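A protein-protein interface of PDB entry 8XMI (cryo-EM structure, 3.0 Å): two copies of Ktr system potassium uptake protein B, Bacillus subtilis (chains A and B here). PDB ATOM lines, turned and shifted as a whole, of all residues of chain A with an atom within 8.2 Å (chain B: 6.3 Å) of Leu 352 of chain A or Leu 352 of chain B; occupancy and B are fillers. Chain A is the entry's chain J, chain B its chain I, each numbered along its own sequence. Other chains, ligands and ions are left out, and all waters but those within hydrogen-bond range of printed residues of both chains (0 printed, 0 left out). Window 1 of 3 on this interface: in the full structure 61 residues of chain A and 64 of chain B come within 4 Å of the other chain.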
ATOM      1  N   ILE A 314      29.973 -17.608  -2.869  1.00  0.00           N
ATOM      2  CA  ILE A 314      28.554 -17.435  -3.133  1.00  0.00           C
ATOM      3  C   ILE A 314      28.330 -15.969  -3.480  1.00  0.00           C
ATOM      4  O   ILE A 314      28.982 -15.068  -2.937  1.00  0.00           O
ATOM      5  CB  ILE A 314      27.673 -17.906  -1.956  1.00  0.00           C
ATOM      6  CG1 ILE A 314      27.403 -16.796  -0.942  1.00  0.00           C
ATOM      7  CG2 ILE A 314      28.310 -19.090  -1.260  1.00  0.00           C
ATOM      8  CD1 ILE A 314      26.324 -17.138   0.040  1.00  0.00           C
ATOM      9  N   THR A 318      22.978 -14.437  -4.487  1.00  0.00           N
ATOM     10  CA  THR A 318      22.635 -15.635  -3.729  1.00  0.00           C
ATOM     11  C   THR A 318      22.386 -15.304  -2.264  1.00  0.00           C
ATOM     12  O   THR A 318      21.470 -15.850  -1.641  1.00  0.00           O
ATOM     13  CB  THR A 318      23.747 -16.676  -3.865  1.00  0.00           C
ATOM     14  OG1 THR A 318      23.912 -17.020  -5.245  1.00  0.00           O
ATOM     15  CG2 THR A 318      23.418 -17.932  -3.084  1.00  0.00           C
ATOM     16  N   VAL A 321      18.962 -13.346  -2.048  1.00  0.00           N
ATOM     17  CA  VAL A 321      17.826 -14.227  -2.314  1.00  0.00           C
ATOM     18  C   VAL A 321      17.528 -15.101  -1.103  1.00  0.00           C
ATOM     19  O   VAL A 321      16.365 -15.290  -0.727  1.00  0.00           O
ATOM     20  CB  VAL A 321      18.090 -15.063  -3.582  1.00  0.00           C
ATOM     21  CG1 VAL A 321      17.323 -16.364  -3.555  1.00  0.00           C
ATOM     22  CG2 VAL A 321      17.715 -14.267  -4.815  1.00  0.00           C
ATOM     23  N   ILE A 322      18.568 -15.638  -0.465  1.00  0.00           N
ATOM     24  CA  ILE A 322      18.370 -16.447   0.734  1.00  0.00           C
ATOM     25  C   ILE A 322      17.911 -15.584   1.901  1.00  0.00           C
ATOM     26  O   ILE A 322      17.008 -15.966   2.652  1.00  0.00           O
ATOM     27  CB  ILE A 322      19.660 -17.212   1.071  1.00  0.00           C
ATOM     28  CG1 ILE A 322      19.905 -18.303   0.039  1.00  0.00           C
ATOM     29  CG2 ILE A 322      19.593 -17.809   2.460  1.00  0.00           C
ATOM     30  CD1 ILE A 322      21.135 -19.096   0.312  1.00  0.00           C
ATOM     31  N   LEU A 323      18.520 -14.410   2.070  1.00  0.00           N
ATOM     32  CA  LEU A 323      18.179 -13.549   3.198  1.00  0.00           C
ATOM     33  C   LEU A 323      16.746 -13.043   3.101  1.00  0.00           C
ATOM     34  O   LEU A 323      16.028 -13.001   4.104  1.00  0.00           O
ATOM     35  CB  LEU A 323      19.152 -12.375   3.264  1.00  0.00           C
ATOM     36  CG  LEU A 323      19.500 -11.859   4.654  1.00  0.00           C
ATOM     37  CD1 LEU A 323      20.243 -12.929   5.425  1.00  0.00           C
ATOM     38  CD2 LEU A 323      20.326 -10.593   4.548  1.00  0.00           C
ATOM     39  N   SER A 325      14.313 -14.515   1.403  1.00  0.00           N
ATOM     40  CA  SER A 325      13.409 -15.654   1.515  1.00  0.00           C
ATOM     41  C   SER A 325      13.122 -15.996   2.971  1.00  0.00           C
ATOM     42  O   SER A 325      11.993 -16.357   3.317  1.00  0.00           O
ATOM     43  CB  SER A 325      13.999 -16.861   0.788  1.00  0.00           C
ATOM     44  OG  SER A 325      13.218 -18.019   1.002  1.00  0.00           O
ATOM     45  N   VAL A 326      14.135 -15.904   3.833  1.00  0.00           N
ATOM     46  CA  VAL A 326      13.938 -16.175   5.253  1.00  0.00           C
ATOM     47  C   VAL A 326      13.132 -15.062   5.907  1.00  0.00           C
ATOM     48  O   VAL A 326      12.196 -15.323   6.667  1.00  0.00           O
ATOM     49  CB  VAL A 326      15.298 -16.373   5.943  1.00  0.00           C
ATOM     50  CG1 VAL A 326      15.118 -16.557   7.435  1.00  0.00           C
ATOM     51  CG2 VAL A 326      16.009 -17.566   5.347  1.00  0.00           C
ATOM     52  N   ILE A 327      13.477 -13.806   5.614  1.00  0.00           N
ATOM     53  CA  ILE A 327      12.821 -12.667   6.254  1.00  0.00           C
ATOM     54  C   ILE A 327      11.354 -12.590   5.852  1.00  0.00           C
ATOM     55  O   ILE A 327      10.485 -12.285   6.677  1.00  0.00           O
ATOM     56  CB  ILE A 327      13.585 -11.373   5.920  1.00  0.00           C
ATOM     57  CG1 ILE A 327      14.915 -11.341   6.673  1.00  0.00           C
ATOM     58  CG2 ILE A 327      12.768 -10.144   6.253  1.00  0.00           C
ATOM     59  CD1 ILE A 327      15.792 -10.173   6.308  1.00  0.00           C
ATOM     60  N   TYR A 329       9.559 -15.187   5.084  1.00  0.00           N
ATOM     61  CA  TYR A 329       8.925 -16.268   5.830  1.00  0.00           C
ATOM     62  C   TYR A 329       8.690 -15.875   7.282  1.00  0.00           C
ATOM     63  O   TYR A 329       7.641 -16.189   7.852  1.00  0.00           O
ATOM     64  CB  TYR A 329       9.777 -17.535   5.747  1.00  0.00           C
ATOM     65  CG  TYR A 329       9.252 -18.677   6.582  1.00  0.00           C
ATOM     66  CD1 TYR A 329       8.202 -19.459   6.136  1.00  0.00           C
ATOM     67  CD2 TYR A 329       9.807 -18.971   7.817  1.00  0.00           C
ATOM     68  CE1 TYR A 329       7.718 -20.500   6.895  1.00  0.00           C
ATOM     69  CE2 TYR A 329       9.330 -20.008   8.582  1.00  0.00           C
ATOM     70  CZ  TYR A 329       8.284 -20.769   8.118  1.00  0.00           C
ATOM     71  OH  TYR A 329       7.804 -21.808   8.878  1.00  0.00           O
ATOM     72  N   TYR A 345      10.390 -20.214  -7.096  1.00  0.00           N
ATOM     73  CA  TYR A 345      11.005 -21.328  -6.378  1.00  0.00           C
ATOM     74  C   TYR A 345      12.264 -21.904  -7.030  1.00  0.00           C
ATOM     75  O   TYR A 345      13.184 -22.268  -6.278  1.00  0.00           O
ATOM     76  CB  TYR A 345       9.953 -22.423  -6.157  1.00  0.00           C
ATOM     77  CG  TYR A 345      10.504 -23.712  -5.594  1.00  0.00           C
ATOM     78  CD1 TYR A 345      10.841 -23.819  -4.252  1.00  0.00           C
ATOM     79  CD2 TYR A 345      10.672 -24.830  -6.403  1.00  0.00           C
ATOM     80  CE1 TYR A 345      11.342 -24.999  -3.732  1.00  0.00           C
ATOM     81  CE2 TYR A 345      11.171 -26.012  -5.893  1.00  0.00           C
ATOM     82  CZ  TYR A 345      11.502 -26.092  -4.558  1.00  0.00           C
ATOM     83  OH  TYR A 345      11.997 -27.269  -4.047  1.00  0.00           O
ATOM     84  N   PRO A 346      12.370 -22.068  -8.362  1.00  0.00           N
ATOM     85  CA  PRO A 346      13.647 -22.550  -8.921  1.00  0.00           C
ATOM     86  C   PRO A 346      14.841 -21.661  -8.620  1.00  0.00           C
ATOM     87  O   PRO A 346      15.972 -22.160  -8.576  1.00  0.00           O
ATOM     88  CB  PRO A 346      13.362 -22.611 -10.426  1.00  0.00           C
ATOM     89  CG  PRO A 346      11.934 -22.870 -10.508  1.00  0.00           C
ATOM     90  CD  PRO A 346      11.321 -22.078  -9.400  1.00  0.00           C
ATOM     91  N   ILE A 347      14.635 -20.358  -8.433  1.00  0.00           N
ATOM     92  CA  ILE A 347      15.735 -19.490  -8.029  1.00  0.00           C
ATOM     93  C   ILE A 347      16.141 -19.780  -6.590  1.00  0.00           C
ATOM     94  O   ILE A 347      17.331 -19.787  -6.257  1.00  0.00           O
ATOM     95  CB  ILE A 347      15.350 -18.014  -8.217  1.00  0.00           C
ATOM     96  CG1 ILE A 347      14.751 -17.781  -9.603  1.00  0.00           C
ATOM     97  CG2 ILE A 347      16.556 -17.126  -8.017  1.00  0.00           C
ATOM     98  CD1 ILE A 347      15.715 -18.009 -10.734  1.00  0.00           C
ATOM     99  N   ILE A 348      15.162 -20.019  -5.716  1.00  0.00           N
ATOM    100  CA  ILE A 348      15.447 -20.216  -4.298  1.00  0.00           C
ATOM    101  C   ILE A 348      16.165 -21.537  -4.068  1.00  0.00           C
ATOM    102  O   ILE A 348      17.087 -21.621  -3.250  1.00  0.00           O
ATOM    103  CB  ILE A 348      14.150 -20.141  -3.472  1.00  0.00           C
ATOM    104  CG1 ILE A 348      13.293 -18.953  -3.905  1.00  0.00           C
ATOM    105  CG2 ILE A 348      14.471 -20.047  -1.995  1.00  0.00           C
ATOM    106  CD1 ILE A 348      13.880 -17.618  -3.569  1.00  0.00           C
ATOM    107  N   ILE A 349      15.843 -22.541  -4.844  1.00  0.00           N
ATOM    108  CA  ILE A 349      16.453 -23.815  -4.630  1.00  0.00           C
ATOM    109  C   ILE A 349      17.903 -23.877  -5.076  1.00  0.00           C
ATOM    110  O   ILE A 349      18.704 -24.508  -4.420  1.00  0.00           O
ATOM    111  CB  ILE A 349      15.646 -24.907  -5.322  1.00  0.00           C
ATOM    112  CG1 ILE A 349      16.182 -26.280  -4.931  1.00  0.00           C
ATOM    113  CG2 ILE A 349      15.687 -24.744  -6.833  1.00  0.00           C
ATOM    114  CD1 ILE A 349      15.323 -27.426  -5.414  1.00  0.00           C
ATOM    115  N   LYS A 350      18.270 -23.247  -6.172  1.00  0.00           N
ATOM    116  CA  LYS A 350      19.652 -23.211  -6.579  1.00  0.00           C
ATOM    117  C   LYS A 350      20.476 -22.470  -5.596  1.00  0.00           C
ATOM    118  O   LYS A 350      21.598 -22.854  -5.329  1.00  0.00           O
ATOM    119  CB  LYS A 350      19.818 -22.571  -7.927  1.00  0.00           C
ATOM    120  CG  LYS A 350      21.174 -22.790  -8.549  1.00  0.00           C
ATOM    121  CD  LYS A 350      21.180 -22.322  -9.982  1.00  0.00           C
ATOM    122  CE  LYS A 350      22.517 -22.609 -10.632  1.00  0.00           C
ATOM    123  NZ  LYS A 350      22.538 -22.168 -12.051  1.00  0.00           N
ATOM    124  N   ALA A 351      19.977 -21.397  -5.059  1.00  0.00           N
ATOM    125  CA  ALA A 351      20.720 -20.598  -4.124  1.00  0.00           C
ATOM    126  C   ALA A 351      21.031 -21.340  -2.896  1.00  0.00           C
ATOM    127  O   ALA A 351      22.124 -21.235  -2.371  1.00  0.00           O
ATOM    128  CB  ALA A 351      19.914 -19.414  -3.740  1.00  0.00           C
ATOM    129  N   LEU A 352      20.088 -22.089  -2.412  1.00  0.00           N
ATOM    130  CA  LEU A 352      20.299 -22.855  -1.256  1.00  0.00           C
ATOM    131  C   LEU A 352      21.360 -23.869  -1.507  1.00  0.00           C
ATOM    132  O   LEU A 352      22.219 -24.054  -0.673  1.00  0.00           O
ATOM    133  CB  LEU A 352      19.007 -23.528  -0.874  1.00  0.00           C
ATOM    134  CG  LEU A 352      19.001 -24.395   0.381  1.00  0.00           C
ATOM    135  CD1 LEU A 352      19.694 -25.732   0.177  1.00  0.00           C
ATOM    136  CD2 LEU A 352      19.655 -23.616   1.501  1.00  0.00           C
ATOM    137  N   ALA A 353      21.358 -24.516  -2.633  1.00  0.00           N
ATOM    138  CA  ALA A 353      22.382 -25.459  -2.949  1.00  0.00           C
ATOM    139  C   ALA A 353      23.730 -24.850  -3.060  1.00  0.00           C
ATOM    140  O   ALA A 353      24.683 -25.415  -2.590  1.00  0.00           O
ATOM    141  CB  ALA A 353      22.045 -26.136  -4.226  1.00  0.00           C
ATOM    142  N   VAL A 354      23.847 -23.691  -3.644  1.00  0.00           N
ATOM    143  CA  VAL A 354      25.104 -23.046  -3.701  1.00  0.00           C
ATOM    144  C   VAL A 354      25.558 -22.710  -2.317  1.00  0.00           C
ATOM    145  O   VAL A 354      26.736 -22.812  -2.061  1.00  0.00           O
ATOM    146  CB  VAL A 354      25.029 -21.784  -4.529  1.00  0.00           C
ATOM    147  CG1 VAL A 354      26.260 -20.928  -4.321  1.00  0.00           C
ATOM    148  CG2 VAL A 354      24.839 -22.116  -5.991  1.00  0.00           C
ATOM    149  N   SER A 355      24.694 -22.327  -1.394  1.00  0.00           N
ATOM    150  CA  SER A 355      25.211 -21.919  -0.092  1.00  0.00           C
ATOM    151  C   SER A 355      25.478 -23.112   0.816  1.00  0.00           C
ATOM    152  O   SER A 355      26.437 -23.099   1.592  1.00  0.00           O
ATOM    153  CB  SER A 355      24.239 -20.955   0.574  1.00  0.00           C
ATOM    154  OG  SER A 355      24.670 -20.646   1.886  1.00  0.00           O
ATOM    155  N   VAL A 356      24.628 -24.137   0.761  1.00  0.00           N
ATOM    156  CA  VAL A 356      24.823 -25.306   1.613  1.00  0.00           C
ATOM    157  C   VAL A 356      26.027 -26.115   1.152  1.00  0.00           C
ATOM    158  O   VAL A 356      26.828 -26.578   1.971  1.00  0.00           O
ATOM    159  CB  VAL A 356      23.541 -26.155   1.653  1.00  0.00           C
ATOM    160  CG1 VAL A 356      23.801 -27.484   2.331  1.00  0.00           C
ATOM    161  CG2 VAL A 356      22.454 -25.406   2.388  1.00  0.00           C
ATOM    162  N   THR A 357      26.179 -26.297  -0.162  1.00  0.00           N
ATOM    163  CA  THR A 357      27.333 -27.026  -0.680  1.00  0.00           C
ATOM    164  C   THR A 357      28.632 -26.284  -0.396  1.00  0.00           C
ATOM    165  O   THR A 357      29.660 -26.911  -0.122  1.00  0.00           O
ATOM    166  CB  THR A 357      27.179 -27.261  -2.180  1.00  0.00           C
ATOM    167  OG1 THR A 357      25.816 -27.578  -2.473  1.00  0.00           O
ATOM    168  CG2 THR A 357      28.059 -28.407  -2.629  1.00  0.00           C
ATOM    169  N   SER A 358      28.609 -24.954  -0.472  1.00  0.00           N
ATOM    170  CA  SER A 358      29.813 -24.172  -0.210  1.00  0.00           C
ATOM    171  C   SER A 358      30.219 -24.242   1.256  1.00  0.00           C
ATOM    172  O   SER A 358      31.410 -24.309   1.569  1.00  0.00           O
ATOM    173  CB  SER A 358      29.598 -22.726  -0.640  1.00  0.00           C
ATOM    174  OG  SER A 358      28.539 -22.142   0.086  1.00  0.00           O
ATOM    175  N   LEU A 359      29.246 -24.212   2.169  1.00  0.00           N
ATOM    176  CA  LEU A 359      29.554 -24.356   3.589  1.00  0.00           C
ATOM    177  C   LEU A 359      30.087 -25.742   3.912  1.00  0.00           C
ATOM    178  O   LEU A 359      30.960 -25.883   4.773  1.00  0.00           O
ATOM    179  CB  LEU A 359      28.317 -24.072   4.433  1.00  0.00           C
ATOM    180  CG  LEU A 359      28.100 -22.641   4.916  1.00  0.00           C
ATOM    181  CD1 LEU A 359      26.896 -22.584   5.831  1.00  0.00           C
ATOM    182  CD2 LEU A 359      29.338 -22.125   5.625  1.00  0.00           C
ATOM    183  N   LEU A 421      28.493 -26.180  -7.685  1.00  0.00           N
ATOM    184  CA  LEU A 421      27.462 -26.853  -8.470  1.00  0.00           C
ATOM    185  C   LEU A 421      28.035 -27.488  -9.729  1.00  0.00           C
ATOM    186  O   LEU A 421      27.743 -28.649 -10.030  1.00  0.00           O
ATOM    187  CB  LEU A 421      26.349 -25.879  -8.845  1.00  0.00           C
ATOM    188  CG  LEU A 421      25.449 -25.324  -7.748  1.00  0.00           C
ATOM    189  CD1 LEU A 421      24.136 -24.871  -8.356  1.00  0.00           C
ATOM    190  CD2 LEU A 421      25.219 -26.351  -6.667  1.00  0.00           C
ATOM    191  N   THR A 444      10.362 -30.347  11.526  1.00  0.00           N
ATOM    192  CA  THR A 444      11.663 -29.715  11.344  1.00  0.00           C
ATOM    193  C   THR A 444      11.779 -28.437  12.165  1.00  0.00           C
ATOM    194  O   THR A 444      12.355 -27.443  11.724  1.00  0.00           O
ATOM    195  CB  THR A 444      11.926 -29.424   9.868  1.00  0.00           C
ATOM    196  OG1 THR A 444      10.911 -28.551   9.363  1.00  0.00           O
ATOM    197  CG2 THR A 444      11.915 -30.710   9.065  1.00  0.00           C
ATOM    198  N   THR B 318      15.824 -31.493  10.857  1.00  0.00           N
ATOM    199  CA  THR B 318      16.131 -30.326  10.036  1.00  0.00           C
ATOM    200  C   THR B 318      17.393 -30.555   9.218  1.00  0.00           C
ATOM    201  O   THR B 318      17.452 -30.199   8.036  1.00  0.00           O
ATOM    202  CB  THR B 318      16.282 -29.089  10.922  1.00  0.00           C
ATOM    203  OG1 THR B 318      15.043 -28.822  11.587  1.00  0.00           O
ATOM    204  CG2 THR B 318      16.675 -27.873  10.105  1.00  0.00           C
ATOM    205  N   ILE B 322      17.517 -30.799   4.950  1.00  0.00           N
ATOM    206  CA  ILE B 322      18.318 -29.902   4.121  1.00  0.00           C
ATOM    207  C   ILE B 322      19.388 -30.676   3.365  1.00  0.00           C
ATOM    208  O   ILE B 322      19.666 -30.394   2.195  1.00  0.00           O
ATOM    209  CB  ILE B 322      18.928 -28.785   4.986  1.00  0.00           C
ATOM    210  CG1 ILE B 322      17.827 -27.968   5.650  1.00  0.00           C
ATOM    211  CG2 ILE B 322      19.795 -27.862   4.155  1.00  0.00           C
ATOM    212  CD1 ILE B 322      18.356 -26.895   6.548  1.00  0.00           C
ATOM    213  N   SER B 325      17.633 -32.595   0.591  1.00  0.00           N
ATOM    214  CA  SER B 325      17.096 -31.704  -0.432  1.00  0.00           C
ATOM    215  C   SER B 325      18.197 -31.174  -1.340  1.00  0.00           C
ATOM    216  O   SER B 325      17.968 -30.949  -2.533  1.00  0.00           O
ATOM    217  CB  SER B 325      16.341 -30.549   0.220  1.00  0.00           C
ATOM    218  OG  SER B 325      16.004 -29.561  -0.732  1.00  0.00           O
ATOM    219  N   VAL B 326      19.391 -30.946  -0.792  1.00  0.00           N
ATOM    220  CA  VAL B 326      20.512 -30.495  -1.611  1.00  0.00           C
ATOM    221  C   VAL B 326      20.998 -31.619  -2.515  1.00  0.00           C
ATOM    222  O   VAL B 326      21.227 -31.412  -3.711  1.00  0.00           O
ATOM    223  CB  VAL B 326      21.640 -29.959  -0.711  1.00  0.00           C
ATOM    224  CG1 VAL B 326      22.926 -29.799  -1.498  1.00  0.00           C
ATOM    225  CG2 VAL B 326      21.234 -28.636  -0.100  1.00  0.00           C
ATOM    226  N   ILE B 347       7.714 -28.038   4.382  1.00  0.00           N
ATOM    227  CA  ILE B 347       8.667 -28.669   5.287  1.00  0.00           C
ATOM    228  C   ILE B 347      10.083 -28.191   4.994  1.00  0.00           C
ATOM    229  O   ILE B 347      10.893 -28.008   5.908  1.00  0.00           O
ATOM    230  CB  ILE B 347       8.551 -30.200   5.192  1.00  0.00           C
ATOM    231  CG1 ILE B 347       7.096 -30.637   5.357  1.00  0.00           C
ATOM    232  CG2 ILE B 347       9.418 -30.871   6.236  1.00  0.00           C
ATOM    233  CD1 ILE B 347       6.507 -30.315   6.706  1.00  0.00           C
ATOM    234  N   ILE B 348      10.408 -27.986   3.716  1.00  0.00           N
ATOM    235  CA  ILE B 348      11.762 -27.594   3.341  1.00  0.00           C
ATOM    236  C   ILE B 348      12.051 -26.161   3.770  1.00  0.00           C
ATOM    237  O   ILE B 348      13.144 -25.856   4.257  1.00  0.00           O
ATOM    238  CB  ILE B 348      11.978 -27.778   1.830  1.00  0.00           C
ATOM    239  CG1 ILE B 348      11.506 -29.159   1.376  1.00  0.00           C
ATOM    240  CG2 ILE B 348      13.441 -27.591   1.480  1.00  0.00           C
ATOM    241  CD1 ILE B 348      12.358 -30.293   1.869  1.00  0.00           C
ATOM    242  N   ILE B 349      11.089 -25.253   3.580  1.00  0.00           N
ATOM    243  CA  ILE B 349      11.345 -23.845   3.868  1.00  0.00           C
ATOM    244  C   ILE B 349      11.444 -23.596   5.370  1.00  0.00           C
ATOM    245  O   ILE B 349      12.220 -22.740   5.809  1.00  0.00           O
ATOM    246  CB  ILE B 349      10.278 -22.953   3.199  1.00  0.00           C
ATOM    247  CG1 ILE B 349      10.617 -21.473   3.389  1.00  0.00           C
ATOM    248  CG2 ILE B 349       8.886 -23.257   3.719  1.00  0.00           C
ATOM    249  CD1 ILE B 349       9.594 -20.532   2.808  1.00  0.00           C
ATOM    250  N   LYS B 350      10.686 -24.331   6.185  1.00  0.00           N
ATOM    251  CA  LYS B 350      10.807 -24.167   7.628  1.00  0.00           C
ATOM    252  C   LYS B 350      12.149 -24.678   8.128  1.00  0.00           C
ATOM    253  O   LYS B 350      12.749 -24.082   9.028  1.00  0.00           O
ATOM    254  CB  LYS B 350       9.665 -24.875   8.348  1.00  0.00           C
ATOM    255  CG  LYS B 350       9.653 -24.607   9.841  1.00  0.00           C
ATOM    256  CD  LYS B 350       8.503 -25.295  10.538  1.00  0.00           C
ATOM    257  CE  LYS B 350       8.547 -25.028  12.030  1.00  0.00           C
ATOM    258  NZ  LYS B 350       7.420 -25.681  12.749  1.00  0.00           N
ATOM    259  N   ALA B 351      12.635 -25.783   7.560  1.00  0.00           N
ATOM    260  CA  ALA B 351      13.967 -26.270   7.905  1.00  0.00           C
ATOM    261  C   ALA B 351      15.038 -25.275   7.487  1.00  0.00           C
ATOM    262  O   ALA B 351      16.029 -25.083   8.199  1.00  0.00           O
ATOM    263  CB  ALA B 351      14.214 -27.627   7.252  1.00  0.00           C
ATOM    264  N   LEU B 352      14.888 -24.530   6.445  1.00  0.00           N
ATOM    265  CA  LEU B 352      15.947 -23.638   6.071  1.00  0.00           C
ATOM    266  C   LEU B 352      15.788 -22.389   6.833  1.00  0.00           C
ATOM    267  O   LEU B 352      16.765 -21.744   7.128  1.00  0.00           O
ATOM    268  CB  LEU B 352      15.948 -23.361   4.582  1.00  0.00           C
ATOM    269  CG  LEU B 352      17.075 -22.559   3.940  1.00  0.00           C
ATOM    270  CD1 LEU B 352      16.867 -21.061   4.088  1.00  0.00           C
ATOM    271  CD2 LEU B 352      18.425 -22.989   4.488  1.00  0.00           C
ATOM    272  N   ALA B 353      14.586 -22.022   7.214  1.00  0.00           N
ATOM    273  CA  ALA B 353      14.474 -20.835   8.053  1.00  0.00           C
ATOM    274  C   ALA B 353      15.107 -21.043   9.421  1.00  0.00           C
ATOM    275  O   ALA B 353      15.688 -20.108   9.977  1.00  0.00           O
ATOM    276  CB  ALA B 353      13.011 -20.432   8.209  1.00  0.00           C
ATOM    277  N   VAL B 354      14.991 -22.248   9.984  1.00  0.00           N
ATOM    278  CA  VAL B 354      15.636 -22.547  11.260  1.00  0.00           C
ATOM    279  C   VAL B 354      17.150 -22.486  11.117  1.00  0.00           C
ATOM    280  O   VAL B 354      17.848 -21.919  11.963  1.00  0.00           O
ATOM    281  CB  VAL B 354      15.177 -23.921  11.783  1.00  0.00           C
ATOM    282  CG1 VAL B 354      15.976 -24.323  13.008  1.00  0.00           C
ATOM    283  CG2 VAL B 354      13.703 -23.901  12.110  1.00  0.00           C
ATOM    284  N   SER B 355      17.678 -23.066  10.038  1.00  0.00           N
ATOM    285  CA  SER B 355      19.124 -23.171   9.874  1.00  0.00           C
ATOM    286  C   SER B 355      19.767 -21.815   9.612  1.00  0.00           C
ATOM    287  O   SER B 355      20.829 -21.513  10.166  1.00  0.00           O
ATOM    288  CB  SER B 355      19.440 -24.144   8.744  1.00  0.00           C
ATOM    289  OG  SER B 355      20.831 -24.211   8.503  1.00  0.00           O
ATOM    290  N   VAL B 356      19.153 -20.990   8.762  1.00  0.00           N
ATOM    291  CA  VAL B 356      19.735 -19.691   8.435  1.00  0.00           C
ATOM    292  C   VAL B 356      19.643 -18.742   9.624  1.00  0.00           C
ATOM    293  O   VAL B 356      20.581 -17.989   9.906  1.00  0.00           O
ATOM    294  CB  VAL B 356      19.062 -19.109   7.179  1.00  0.00           C
ATOM    295  CG1 VAL B 356      19.551 -17.701   6.909  1.00  0.00           C
ATOM    296  CG2 VAL B 356      19.345 -19.985   5.984  1.00  0.00           C
ATOM    297  N   THR B 357      18.516 -18.758  10.336  1.00  0.00           N
ATOM    298  CA  THR B 357      18.372 -17.909  11.515  1.00  0.00           C
ATOM    299  C   THR B 357      19.343 -18.319  12.613  1.00  0.00           C
ATOM    300  O   THR B 357      19.897 -17.463  13.312  1.00  0.00           O
ATOM    301  CB  THR B 357      16.937 -17.963  12.031  1.00  0.00           C
ATOM    302  OG1 THR B 357      16.031 -17.834  10.932  1.00  0.00           O
ATOM    303  CG2 THR B 357      16.682 -16.841  13.009  1.00  0.00           C
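The side-chain hydroxyl of Thr 318 of chain B sits at hydrogen-bond distance from the backbone carbonyl oxygen of Thr 444 of chain A, at 3.0 Å. The backbone carbonyl oxygen of Ile 347 of chain B lies within hydrogen-bond range of the side-chain hydroxyl of Thr 444 of chain A (3.5 Å).
The backbone carbonyl oxygen (O) of Ala 353 of chain B is in hydrogen-bond range of the side-chain hydroxyl (OG1) of Thr 357 of chain B (2.5 Å). O of Ala 353 of chain A is in hydrogen-bond range of OG1 of Thr 357 of chain A (2.4 Å).
Among the printed residues, pairs that only touch across the chains: Val 326 of chain A with Leu 352 of chain B (3.8 Å), Val 326 of chain A with Val 356 of chain B (3.9 Å), Val 326 of chain A with Thr 357 of chain B (3.8 Å), Tyr 329 of chain A with Ile 349 of chain B (3.8 Å), Tyr 329 of chain A with Lys 350 of chain B (3.5 Å), Tyr 329 of chain A with Ala 353 of chain B (3.5 Å), Leu 352 of chain A with Val 326 of chain B (3.3 Å), Leu 352 of chain A with Leu 352 of chain B (3.3 Å), Val 356 of chain A with Val 326 of chain B (3.7 Å), Thr 357 of chain A with Val 326 of chain B (3.8 Å), Thr 444 of chain A with Ala 351 of chain B (3.7 Å) and Thr 444 of chain A with Val 354 of chain B (3.8 Å).
Printed residues of chain B within 4 Å of Val 326 of chain A: Leu 352 (3.8 Å), Val 356 (3.9 Å) and Thr 357 (3.8 Å). Leu 352 of chain A touches just these residues of chain B: Val 326 (3.3 Å) and Leu 352 (3.3 Å). Ala 353 of chain A touches none of the printed residues of chain B. Of the printed residues of chain B, Thr 357 of chain A touches Val 326. Printed residues of chain A within 4 Å of Val 326 of chain B: Leu 352, Val 356 and Thr 357. Of the printed residues of chain A, Ile 349 of chain B touches Tyr 329. Ala 351 of chain B touches one residue of chain A. Of chain A, only Val 326 (3.8 Å) and Leu 352 (3.3 Å) come within 4 Å of Leu 352 of chain B. Printed residues of chain A within 4 Å of Val 356 of chain B: Val 326 (3.9 Å). The nearest residue of chain B that does not touch Leu 352 of chain A is Ile 322 of chain B (4.5 Å). The nearest printed residue of chain A that does not touch Val 326 of chain B is Ala 353 of chain A (4.4 Å).
Along chain B the printed residues that touch a printed residue of chain A span positions 318 to 357. Among the printed residues, 14 pairs touch across the chains.
Val 326 of chain A touches Leu 352 of chain B, and with the chains exchanged Leu 352 of chain A touches Val 326 of chain B. Val 326 of chain A touches Val 356 of chain B, and with the chains exchanged Val 356 of chain A touches Val 326 of chain B. Val 326 of chain A touches Thr 357 of chain B, and with the chains exchanged Thr 357 of chain A touches Val 326 of chain B. Leu 352 of chain B touches its own counterpart, Leu 352 of chain A. Of the 14 pairs that touch across the chains among the printed residues, 7 have their exchanged pair printed and touching as well.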
